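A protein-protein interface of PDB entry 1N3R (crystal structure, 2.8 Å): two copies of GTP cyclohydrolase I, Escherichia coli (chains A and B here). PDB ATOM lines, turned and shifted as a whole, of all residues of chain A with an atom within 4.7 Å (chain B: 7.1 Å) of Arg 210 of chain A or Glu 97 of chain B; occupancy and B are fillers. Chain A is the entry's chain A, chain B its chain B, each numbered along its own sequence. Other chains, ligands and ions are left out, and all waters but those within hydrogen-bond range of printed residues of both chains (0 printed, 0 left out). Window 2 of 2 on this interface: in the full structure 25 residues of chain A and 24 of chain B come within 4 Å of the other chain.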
ATOM      1  N   THR A 197       3.394  18.476  -9.875  1.00  0.00           N
ATOM      2  CA  THR A 197       4.214  19.670 -10.124  1.00  0.00           C
ATOM      3  C   THR A 197       5.714  19.436  -9.897  1.00  0.00           C
ATOM      4  O   THR A 197       6.109  18.689  -9.015  1.00  0.00           O
ATOM      5  CB  THR A 197       3.745  20.900  -9.268  1.00  0.00           C
ATOM      6  OG1 THR A 197       4.804  21.316  -8.389  1.00  0.00           O
ATOM      7  CG2 THR A 197       2.485  20.560  -8.455  1.00  0.00           C
ATOM      8  N   SER A 198       6.535  20.078 -10.721  1.00  0.00           N
ATOM      9  CA  SER A 198       7.989  19.974 -10.627  1.00  0.00           C
ATOM     10  C   SER A 198       8.541  21.379 -10.627  1.00  0.00           C
ATOM     11  O   SER A 198       8.435  22.103 -11.619  1.00  0.00           O
ATOM     12  CB  SER A 198       8.570  19.214 -11.816  1.00  0.00           C
ATOM     13  OG  SER A 198       8.114  17.873 -11.832  1.00  0.00           O
ATOM     14  N   LEU A 199       9.124  21.757  -9.497  1.00  0.00           N
ATOM     15  CA  LEU A 199       9.684  23.083  -9.316  1.00  0.00           C
ATOM     16  C   LEU A 199      11.200  23.022  -9.334  1.00  0.00           C
ATOM     17  O   LEU A 199      11.806  22.260  -8.589  1.00  0.00           O
ATOM     18  CB  LEU A 199       9.194  23.657  -7.980  1.00  0.00           C
ATOM     19  CG  LEU A 199       7.676  23.572  -7.771  1.00  0.00           C
ATOM     20  CD1 LEU A 199       7.294  23.879  -6.330  1.00  0.00           C
ATOM     21  CD2 LEU A 199       7.004  24.521  -8.751  1.00  0.00           C
ATOM     22  N   LEU A 202      14.849  28.635  -8.552  1.00  0.00           N
ATOM     23  CA  LEU A 202      14.196  29.531  -7.608  1.00  0.00           C
ATOM     24  C   LEU A 202      12.781  29.089  -7.217  1.00  0.00           C
ATOM     25  O   LEU A 202      12.367  29.257  -6.067  1.00  0.00           O
ATOM     26  CB  LEU A 202      14.156  30.938  -8.201  1.00  0.00           C
ATOM     27  CG  LEU A 202      15.483  31.693  -8.256  1.00  0.00           C
ATOM     28  CD1 LEU A 202      15.339  32.971  -9.075  1.00  0.00           C
ATOM     29  CD2 LEU A 202      15.918  32.011  -6.836  1.00  0.00           C
ATOM     30  N   PHE A 203      12.049  28.515  -8.170  1.00  0.00           N
ATOM     31  CA  PHE A 203      10.681  28.047  -7.927  1.00  0.00           C
ATOM     32  C   PHE A 203      10.608  27.071  -6.767  1.00  0.00           C
ATOM     33  O   PHE A 203       9.527  26.770  -6.265  1.00  0.00           O
ATOM     34  CB  PHE A 203      10.120  27.378  -9.179  1.00  0.00           C
ATOM     35  CG  PHE A 203       9.893  28.322 -10.309  1.00  0.00           C
ATOM     36  CD1 PHE A 203       8.834  29.225 -10.268  1.00  0.00           C
ATOM     37  CD2 PHE A 203      10.753  28.336 -11.400  1.00  0.00           C
ATOM     38  CE1 PHE A 203       8.639  30.129 -11.296  1.00  0.00           C
ATOM     39  CE2 PHE A 203      10.568  29.238 -12.436  1.00  0.00           C
ATOM     40  CZ  PHE A 203       9.506  30.140 -12.385  1.00  0.00           C
ATOM     41  N   LYS A 204      11.764  26.582  -6.340  1.00  0.00           N
ATOM     42  CA  LYS A 204      11.827  25.633  -5.247  1.00  0.00           C
ATOM     43  C   LYS A 204      12.499  26.299  -4.057  1.00  0.00           C
ATOM     44  O   LYS A 204      11.918  26.381  -2.978  1.00  0.00           O
ATOM     45  CB  LYS A 204      12.620  24.408  -5.691  1.00  0.00           C
ATOM     46  CG  LYS A 204      12.377  23.145  -4.888  1.00  0.00           C
ATOM     47  CD  LYS A 204      13.232  22.026  -5.459  1.00  0.00           C
ATOM     48  CE  LYS A 204      13.009  20.704  -4.759  1.00  0.00           C
ATOM     49  NZ  LYS A 204      13.842  19.633  -5.385  1.00  0.00           N
ATOM     50  N   SER A 206      13.551  29.664  -3.576  1.00  0.00           N
ATOM     51  CA  SER A 206      12.935  30.936  -3.213  1.00  0.00           C
ATOM     52  C   SER A 206      11.482  30.721  -2.813  1.00  0.00           C
ATOM     53  O   SER A 206      10.640  30.439  -3.656  1.00  0.00           O
ATOM     54  CB  SER A 206      13.017  31.904  -4.400  1.00  0.00           C
ATOM     55  OG  SER A 206      12.285  33.095  -4.168  1.00  0.00           O
ATOM     56  N   GLN A 207      11.195  30.853  -1.524  1.00  0.00           N
ATOM     57  CA  GLN A 207       9.839  30.681  -1.002  1.00  0.00           C
ATOM     58  C   GLN A 207       8.841  31.627  -1.674  1.00  0.00           C
ATOM     59  O   GLN A 207       7.692  31.265  -1.923  1.00  0.00           O
ATOM     60  CB  GLN A 207       9.839  30.927   0.512  1.00  0.00           C
ATOM     61  CG  GLN A 207       8.479  30.846   1.188  1.00  0.00           C
ATOM     62  CD  GLN A 207       7.960  29.431   1.284  1.00  0.00           C
ATOM     63  OE1 GLN A 207       7.841  28.732   0.278  1.00  0.00           O
ATOM     64  NE2 GLN A 207       7.642  28.999   2.501  1.00  0.00           N
ATOM     65  N   ASN A 208       9.306  32.836  -1.968  1.00  0.00           N
ATOM     66  CA  ASN A 208       8.493  33.871  -2.597  1.00  0.00           C
ATOM     67  C   ASN A 208       8.137  33.581  -4.059  1.00  0.00           C
ATOM     68  O   ASN A 208       7.000  33.794  -4.475  1.00  0.00           O
ATOM     69  CB  ASN A 208       9.216  35.220  -2.475  1.00  0.00           C
ATOM     70  CG  ASN A 208       8.646  36.281  -3.400  1.00  0.00           C
ATOM     71  OD1 ASN A 208       7.430  36.444  -3.504  1.00  0.00           O
ATOM     72  ND2 ASN A 208       9.527  37.018  -4.073  1.00  0.00           N
ATOM     73  N   THR A 209       9.114  33.113  -4.832  1.00  0.00           N
ATOM     74  CA  THR A 209       8.929  32.784  -6.250  1.00  0.00           C
ATOM     75  C   THR A 209       7.959  31.611  -6.427  1.00  0.00           C
ATOM     76  O   THR A 209       7.120  31.613  -7.325  1.00  0.00           O
ATOM     77  CB  THR A 209      10.286  32.398  -6.901  1.00  0.00           C
ATOM     78  OG1 THR A 209      11.173  33.519  -6.855  1.00  0.00           O
ATOM     79  CG2 THR A 209      10.106  31.975  -8.337  1.00  0.00           C
ATOM     80  N   ARG A 210       8.102  30.614  -5.560  1.00  0.00           N
ATOM     81  CA  ARG A 210       7.293  29.389  -5.550  1.00  0.00           C
ATOM     82  C   ARG A 210       5.775  29.645  -5.508  1.00  0.00           C
ATOM     83  O   ARG A 210       4.998  29.107  -6.309  1.00  0.00           O
ATOM     84  CB  ARG A 210       7.704  28.558  -4.326  1.00  0.00           C
ATOM     85  CG  ARG A 210       7.284  27.109  -4.324  1.00  0.00           C
ATOM     86  CD  ARG A 210       7.450  26.558  -2.924  1.00  0.00           C
ATOM     87  NE  ARG A 210       7.241  25.117  -2.853  1.00  0.00           N
ATOM     88  CZ  ARG A 210       8.202  24.220  -3.039  1.00  0.00           C
ATOM     89  NH1 ARG A 210       9.441  24.618  -3.309  1.00  0.00           N
ATOM     90  NH2 ARG A 210       7.925  22.923  -2.965  1.00  0.00           N
ATOM     91  N   HIS A 211       5.358  30.469  -4.556  1.00  0.00           N
ATOM     92  CA  HIS A 211       3.950  30.767  -4.415  1.00  0.00           C
ATOM     93  C   HIS A 211       3.423  31.630  -5.545  1.00  0.00           C
ATOM     94  O   HIS A 211       2.261  31.502  -5.929  1.00  0.00           O
ATOM     95  CB  HIS A 211       3.690  31.373  -3.040  1.00  0.00           C
ATOM     96  CG  HIS A 211       3.712  30.355  -1.942  1.00  0.00           C
ATOM     97  ND1 HIS A 211       3.770  30.694  -0.610  1.00  0.00           N
ATOM     98  CD2 HIS A 211       3.679  29.000  -1.986  1.00  0.00           C
ATOM     99  CE1 HIS A 211       3.773  29.593   0.122  1.00  0.00           C
ATOM    100  NE2 HIS A 211       3.718  28.551  -0.690  1.00  0.00           N
ATOM    101  N   GLU A 212       4.280  32.479  -6.104  1.00  0.00           N
ATOM    102  CA  GLU A 212       3.867  33.324  -7.222  1.00  0.00           C
ATOM    103  C   GLU A 212       3.416  32.418  -8.356  1.00  0.00           C
ATOM    104  O   GLU A 212       2.452  32.720  -9.051  1.00  0.00           O
ATOM    105  CB  GLU A 212       5.017  34.208  -7.722  1.00  0.00           C
ATOM    106  CG  GLU A 212       5.249  35.473  -6.921  1.00  0.00           C
ATOM    107  CD  GLU A 212       6.332  36.355  -7.533  1.00  0.00           C
ATOM    108  OE1 GLU A 212       6.180  36.771  -8.707  1.00  0.00           O
ATOM    109  OE2 GLU A 212       7.334  36.636  -6.838  1.00  0.00           O
ATOM    110  N   PHE A 213       4.120  31.298  -8.510  1.00  0.00           N
ATOM    111  CA  PHE A 213       3.830  30.309  -9.546  1.00  0.00           C
ATOM    112  C   PHE A 213       2.648  29.433  -9.152  1.00  0.00           C
ATOM    113  O   PHE A 213       1.633  29.384  -9.845  1.00  0.00           O
ATOM    114  CB  PHE A 213       5.052  29.415  -9.782  1.00  0.00           C
ATOM    115  CG  PHE A 213       4.782  28.260 -10.693  1.00  0.00           C
ATOM    116  CD1 PHE A 213       4.610  28.459 -12.057  1.00  0.00           C
ATOM    117  CD2 PHE A 213       4.643  26.980 -10.181  1.00  0.00           C
ATOM    118  CE1 PHE A 213       4.296  27.400 -12.900  1.00  0.00           C
ATOM    119  CE2 PHE A 213       4.330  25.917 -11.012  1.00  0.00           C
ATOM    120  CZ  PHE A 213       4.154  26.125 -12.375  1.00  0.00           C
ATOM    121  N   LEU A 214       2.797  28.719  -8.045  1.00  0.00           N
ATOM    122  CA  LEU A 214       1.738  27.837  -7.579  1.00  0.00           C
ATOM    123  C   LEU A 214       0.358  28.486  -7.484  1.00  0.00           C
ATOM    124  O   LEU A 214      -0.651  27.848  -7.770  1.00  0.00           O
ATOM    125  CB  LEU A 214       2.115  27.246  -6.224  1.00  0.00           C
ATOM    126  CG  LEU A 214       3.281  26.263  -6.204  1.00  0.00           C
ATOM    127  CD1 LEU A 214       3.527  25.805  -4.779  1.00  0.00           C
ATOM    128  CD2 LEU A 214       2.968  25.083  -7.125  1.00  0.00           C
ATOM    129  N   LYS B  94      12.425  10.239  -8.613  1.00  0.00           N
ATOM    130  CA  LYS B  94      12.870  11.060  -7.493  1.00  0.00           C
ATOM    131  C   LYS B  94      11.933  12.264  -7.322  1.00  0.00           C
ATOM    132  O   LYS B  94      12.379  13.411  -7.233  1.00  0.00           O
ATOM    133  CB  LYS B  94      14.313  11.540  -7.691  1.00  0.00           C
ATOM    134  CG  LYS B  94      15.392  10.515  -7.325  1.00  0.00           C
ATOM    135  CD  LYS B  94      15.739   9.603  -8.489  1.00  0.00           C
ATOM    136  CE  LYS B  94      16.925   8.699  -8.159  1.00  0.00           C
ATOM    137  NZ  LYS B  94      17.372   7.895  -9.344  1.00  0.00           N
ATOM    138  N   VAL B  95      10.630  11.987  -7.299  1.00  0.00           N
ATOM    139  CA  VAL B  95       9.609  13.018  -7.129  1.00  0.00           C
ATOM    140  C   VAL B  95       9.548  13.424  -5.661  1.00  0.00           C
ATOM    141  O   VAL B  95       9.003  12.704  -4.818  1.00  0.00           O
ATOM    142  CB  VAL B  95       8.217  12.515  -7.571  1.00  0.00           C
ATOM    143  CG1 VAL B  95       7.181  13.604  -7.375  1.00  0.00           C
ATOM    144  CG2 VAL B  95       8.263  12.079  -9.024  1.00  0.00           C
ATOM    145  N   ASP B  96      10.122  14.583  -5.368  1.00  0.00           N
ATOM    146  CA  ASP B  96      10.164  15.101  -4.014  1.00  0.00           C
ATOM    147  C   ASP B  96       9.101  16.174  -3.801  1.00  0.00           C
ATOM    148  O   ASP B  96       9.080  16.832  -2.763  1.00  0.00           O
ATOM    149  CB  ASP B  96      11.556  15.664  -3.718  1.00  0.00           C
ATOM    150  CG  ASP B  96      12.025  16.645  -4.776  1.00  0.00           C
ATOM    151  OD1 ASP B  96      12.221  16.223  -5.935  1.00  0.00           O
ATOM    152  OD2 ASP B  96      12.195  17.838  -4.454  1.00  0.00           O
ATOM    153  N   GLU B  97       8.237  16.359  -4.798  1.00  0.00           N
ATOM    154  CA  GLU B  97       7.151  17.338  -4.716  1.00  0.00           C
ATOM    155  C   GLU B  97       5.852  16.597  -4.446  1.00  0.00           C
ATOM    156  O   GLU B  97       5.779  15.390  -4.650  1.00  0.00           O
ATOM    157  CB  GLU B  97       7.021  18.134  -6.016  1.00  0.00           C
ATOM    158  CG  GLU B  97       8.070  19.239  -6.212  1.00  0.00           C
ATOM    159  CD  GLU B  97       8.105  20.235  -5.060  1.00  0.00           C
ATOM    160  OE1 GLU B  97       7.022  20.545  -4.514  1.00  0.00           O
ATOM    161  OE2 GLU B  97       9.210  20.714  -4.708  1.00  0.00           O
ATOM    162  N   MET B  98       4.822  17.308  -4.000  1.00  0.00           N
ATOM    163  CA  MET B  98       3.552  16.661  -3.692  1.00  0.00           C
ATOM    164  C   MET B  98       2.700  16.295  -4.896  1.00  0.00           C
ATOM    165  O   MET B  98       2.656  17.022  -5.886  1.00  0.00           O
ATOM    166  CB  MET B  98       2.734  17.528  -2.735  1.00  0.00           C
ATOM    167  CG  MET B  98       2.464  18.926  -3.215  1.00  0.00           C
ATOM    168  SD  MET B  98       1.549  19.832  -1.964  1.00  0.00           S
ATOM    169  CE  MET B  98      -0.141  19.779  -2.662  1.00  0.00           C
ATOM    170  N   VAL B  99       2.043  15.139  -4.799  1.00  0.00           N
ATOM    171  CA  VAL B  99       1.157  14.634  -5.840  1.00  0.00           C
ATOM    172  C   VAL B  99      -0.261  14.709  -5.259  1.00  0.00           C
ATOM    173  O   VAL B  99      -0.573  14.109  -4.220  1.00  0.00           O
ATOM    174  CB  VAL B  99       1.521  13.176  -6.238  1.00  0.00           C
ATOM    175  CG1 VAL B  99       0.497  12.625  -7.188  1.00  0.00           C
ATOM    176  CG2 VAL B  99       2.878  13.147  -6.913  1.00  0.00           C
ATOM    177  N   THR B 100      -1.114  15.445  -5.962  1.00  0.00           N
ATOM    178  CA  THR B 100      -2.482  15.688  -5.538  1.00  0.00           C
ATOM    179  C   THR B 100      -3.592  15.079  -6.400  1.00  0.00           C
ATOM    180  O   THR B 100      -3.545  15.128  -7.631  1.00  0.00           O
ATOM    181  CB  THR B 100      -2.706  17.189  -5.477  1.00  0.00           C
ATOM    182  OG1 THR B 100      -1.507  17.810  -4.997  1.00  0.00           O
ATOM    183  CG2 THR B 100      -3.864  17.522  -4.560  1.00  0.00           C
ATOM    184  N   TYR B 125       0.157  13.715  -1.097  1.00  0.00           N
ATOM    185  CA  TYR B 125       1.245  13.063  -0.389  1.00  0.00           C
ATOM    186  C   TYR B 125       2.543  13.381  -1.094  1.00  0.00           C
ATOM    187  O   TYR B 125       2.532  13.714  -2.283  1.00  0.00           O
ATOM    188  CB  TYR B 125       1.053  11.549  -0.344  1.00  0.00           C
ATOM    189  CG  TYR B 125       1.362  10.817  -1.629  1.00  0.00           C
ATOM    190  CD1 TYR B 125       0.406  10.699  -2.631  1.00  0.00           C
ATOM    191  CD2 TYR B 125       2.607  10.216  -1.828  1.00  0.00           C
ATOM    192  CE1 TYR B 125       0.676   9.998  -3.803  1.00  0.00           C
ATOM    193  CE2 TYR B 125       2.895   9.514  -2.992  1.00  0.00           C
ATOM    194  CZ  TYR B 125       1.922   9.406  -3.978  1.00  0.00           C
ATOM    195  OH  TYR B 125       2.174   8.702  -5.135  1.00  0.00           O
ATOM    196  N   ILE B 126       3.655  13.303  -0.363  1.00  0.00           N
ATOM    197  CA  ILE B 126       4.967  13.545  -0.953  1.00  0.00           C
ATOM    198  C   ILE B 126       5.684  12.198  -0.988  1.00  0.00           C
ATOM    199  O   ILE B 126       6.004  11.618   0.061  1.00  0.00           O
ATOM    200  CB  ILE B 126       5.781  14.582  -0.165  1.00  0.00           C
ATOM    201  CG1 ILE B 126       5.113  15.954  -0.286  1.00  0.00           C
ATOM    202  CG2 ILE B 126       7.186  14.667  -0.723  1.00  0.00           C
ATOM    203  CD1 ILE B 126       5.880  17.093   0.357  1.00  0.00           C
ATOM    204  N   PRO B 127       5.929  11.680  -2.207  1.00  0.00           N
ATOM    205  CA  PRO B 127       6.591  10.401  -2.467  1.00  0.00           C
ATOM    206  C   PRO B 127       7.930  10.220  -1.787  1.00  0.00           C
ATOM    207  O   PRO B 127       8.819  11.068  -1.912  1.00  0.00           O
ATOM    208  CB  PRO B 127       6.747  10.394  -3.991  1.00  0.00           C
ATOM    209  CG  PRO B 127       5.632  11.249  -4.464  1.00  0.00           C
ATOM    210  CD  PRO B 127       5.663  12.384  -3.476  1.00  0.00           C
ATOM    211  N   PHE B 203       2.806  18.536   5.808  1.00  0.00           N
ATOM    212  CA  PHE B 203       1.524  19.224   5.612  1.00  0.00           C
ATOM    213  C   PHE B 203       1.030  19.842   6.922  1.00  0.00           C
ATOM    214  O   PHE B 203       0.063  20.609   6.957  1.00  0.00           O
ATOM    215  CB  PHE B 203       0.491  18.255   5.039  1.00  0.00           C
ATOM    216  CG  PHE B 203       0.783  17.835   3.631  1.00  0.00           C
ATOM    217  CD1 PHE B 203       0.469  18.670   2.567  1.00  0.00           C
ATOM    218  CD2 PHE B 203       1.389  16.605   3.364  1.00  0.00           C
ATOM    219  CE1 PHE B 203       0.750  18.290   1.247  1.00  0.00           C
ATOM    220  CE2 PHE B 203       1.679  16.208   2.051  1.00  0.00           C
ATOM    221  CZ  PHE B 203       1.358  17.054   0.990  1.00  0.00           C
ATOM    222  N   ASN B 208       4.871  26.276   5.014  1.00  0.00           N
ATOM    223  CA  ASN B 208       4.983  26.473   3.579  1.00  0.00           C
ATOM    224  C   ASN B 208       4.096  25.469   2.839  1.00  0.00           C
ATOM    225  O   ASN B 208       3.082  25.833   2.235  1.00  0.00           O
ATOM    226  CB  ASN B 208       6.446  26.296   3.161  1.00  0.00           C
ATOM    227  CG  ASN B 208       6.609  26.018   1.676  1.00  0.00           C
ATOM    228  OD1 ASN B 208       6.185  26.805   0.830  1.00  0.00           O
ATOM    229  ND2 ASN B 208       7.230  24.888   1.352  1.00  0.00           N
ATOM    230  N   THR B 209       4.487  24.202   2.909  1.00  0.00           N
ATOM    231  CA  THR B 209       3.785  23.102   2.259  1.00  0.00           C
ATOM    232  C   THR B 209       2.332  22.978   2.700  1.00  0.00           C
ATOM    233  O   THR B 209       1.463  22.681   1.889  1.00  0.00           O
ATOM    234  CB  THR B 209       4.528  21.774   2.524  1.00  0.00           C
ATOM    235  OG1 THR B 209       5.826  21.835   1.913  1.00  0.00           O
ATOM    236  CG2 THR B 209       3.738  20.578   1.978  1.00  0.00           C
ATOM    237  N   GLU B 212       0.242  25.298   0.748  1.00  0.00           N
ATOM    238  CA  GLU B 212       0.333  24.966  -0.671  1.00  0.00           C
ATOM    239  C   GLU B 212      -0.746  23.944  -0.961  1.00  0.00           C
ATOM    240  O   GLU B 212      -1.269  23.874  -2.073  1.00  0.00           O
ATOM    241  CB  GLU B 212       1.697  24.369  -1.009  1.00  0.00           C
ATOM    242  CG  GLU B 212       2.701  25.384  -1.504  1.00  0.00           C
ATOM    243  CD  GLU B 212       4.044  24.766  -1.843  1.00  0.00           C
ATOM    244  OE1 GLU B 212       4.061  23.688  -2.473  1.00  0.00           O
ATOM    245  OE2 GLU B 212       5.080  25.367  -1.487  1.00  0.00           O
ATOM    246  N   ARG B 215      -4.414  25.763  -0.118  1.00  0.00           N
ATOM    247  CA  ARG B 215      -4.742  26.726  -1.156  1.00  0.00           C
ATOM    248  C   ARG B 215      -5.262  25.978  -2.379  1.00  0.00           C
ATOM    249  O   ARG B 215      -6.074  26.501  -3.136  1.00  0.00           O
ATOM    250  CB  ARG B 215      -3.503  27.531  -1.543  1.00  0.00           C
ATOM    251  CG  ARG B 215      -3.695  28.452  -2.743  1.00  0.00           C
ATOM    252  CD  ARG B 215      -2.378  28.655  -3.474  1.00  0.00           C
ATOM    253  NE  ARG B 215      -1.830  27.382  -3.944  1.00  0.00           N
ATOM    254  CZ  ARG B 215      -0.603  26.940  -3.675  1.00  0.00           C
ATOM    255  NH1 ARG B 215       0.229  27.665  -2.933  1.00  0.00           N
ATOM    256  NH2 ARG B 215      -0.210  25.759  -4.137  1.00  0.00           N
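Among the printed residues, merely in contact across the chains: Leu 214 of chain A with Glu 212 of chain B, Thr 197 of chain A with Glu 97 of chain B, His 211 of chain A with Glu 212 of chain B, Leu 214 of chain A with Arg 215 of chain B, Lys 204 of chain A with Glu 97 of chain B, Leu 199 of chain A with Glu 97 of chain B, His 211 of chain A with Arg 215 of chain B and Arg 210 of chain A with Asn 208 of chain B.
Arg 210 of chain A touches just these residues of chain B: Glu 97 (3.0 Å), Asn 208 (3.97 Å) and Glu 212 (2.6 Å).
Phe 213 of chain A touches none of the printed residues of chain B.
Of the printed residues of chain B, Leu 214 of chain A touches Glu 212 and Arg 215.
Of the printed residues of chain A, Asp 96 of chain B touches Lys 204.
Of chain A, only Thr 197 (3.2 Å), Leu 199 (3.8 Å), Lys 204 (3.8 Å) and Arg 210 (3.0 Å) come within 4 Å of Glu 97 of chain B.
The nearest printed residue of chain B that does not touch Leu 199 of chain A is Glu 212 of chain B (5.0 Å).
The side-chain amide nitrogen of Asn 208 of chain B is in hydrogen-bond range of the side-chain hydroxyl of Thr 209 of chain B (3.4 Å).
The backbone carbonyl oxygen (O) of Lys 204 of chain A sits at hydrogen-bond distance from the guanidinium group (NH1) of Arg 210 of chain A (3.1 Å).
OE2 of Glu 212 of chain B sits close to OD1 of Asn 208 of chain B (2.9 Å).
O of Glu 212 of chain B is in hydrogen-bond range of NH2 of Arg 215 of chain B (3.0 Å).
OE1 of Glu 97 of chain B is in salt-bridge range of NH2 of Arg 210 of chain A, at 3.0 Å.
OE1 of Gln 207 of chain A lies close to OD1 of Asn 208 of chain B, 2.6 Å away.
A ring nitrogen (NE2) of His 211 of chain A lies within hydrogen-bond range of the side-chain amide oxygen of Asn 208 of chain B (3.4 Å).
The guanidinium group (NE) of Arg 210 of chain A lies within salt-bridge range of the side-chain carboxylate (OE2) of Glu 212 of chain B (2.6 Å).
OD2 of Asp 96 of chain B is in salt-bridge range of NZ of Lys 204 of chain A (2.6 Å).
Along chain B the printed residues that touch a printed residue of chain A span positions 96 to 215.
Among the printed residues, Asp or Glu carboxylates within 4 Å of a Lys or Arg side-chain nitrogen of the other chain: Lys 204 of chain A with Asp 96 of chain B (2.6 Å), Arg 210 of chain A with Glu 97 of chain B (3.0 Å) and Arg 210 of chain A with Glu 212 of chain B (2.6 Å).
4 positions are printed for both chains.
Of the 13 pairs that touch across the chains among the printed residues, none has its exchanged pair printed and touching as well.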
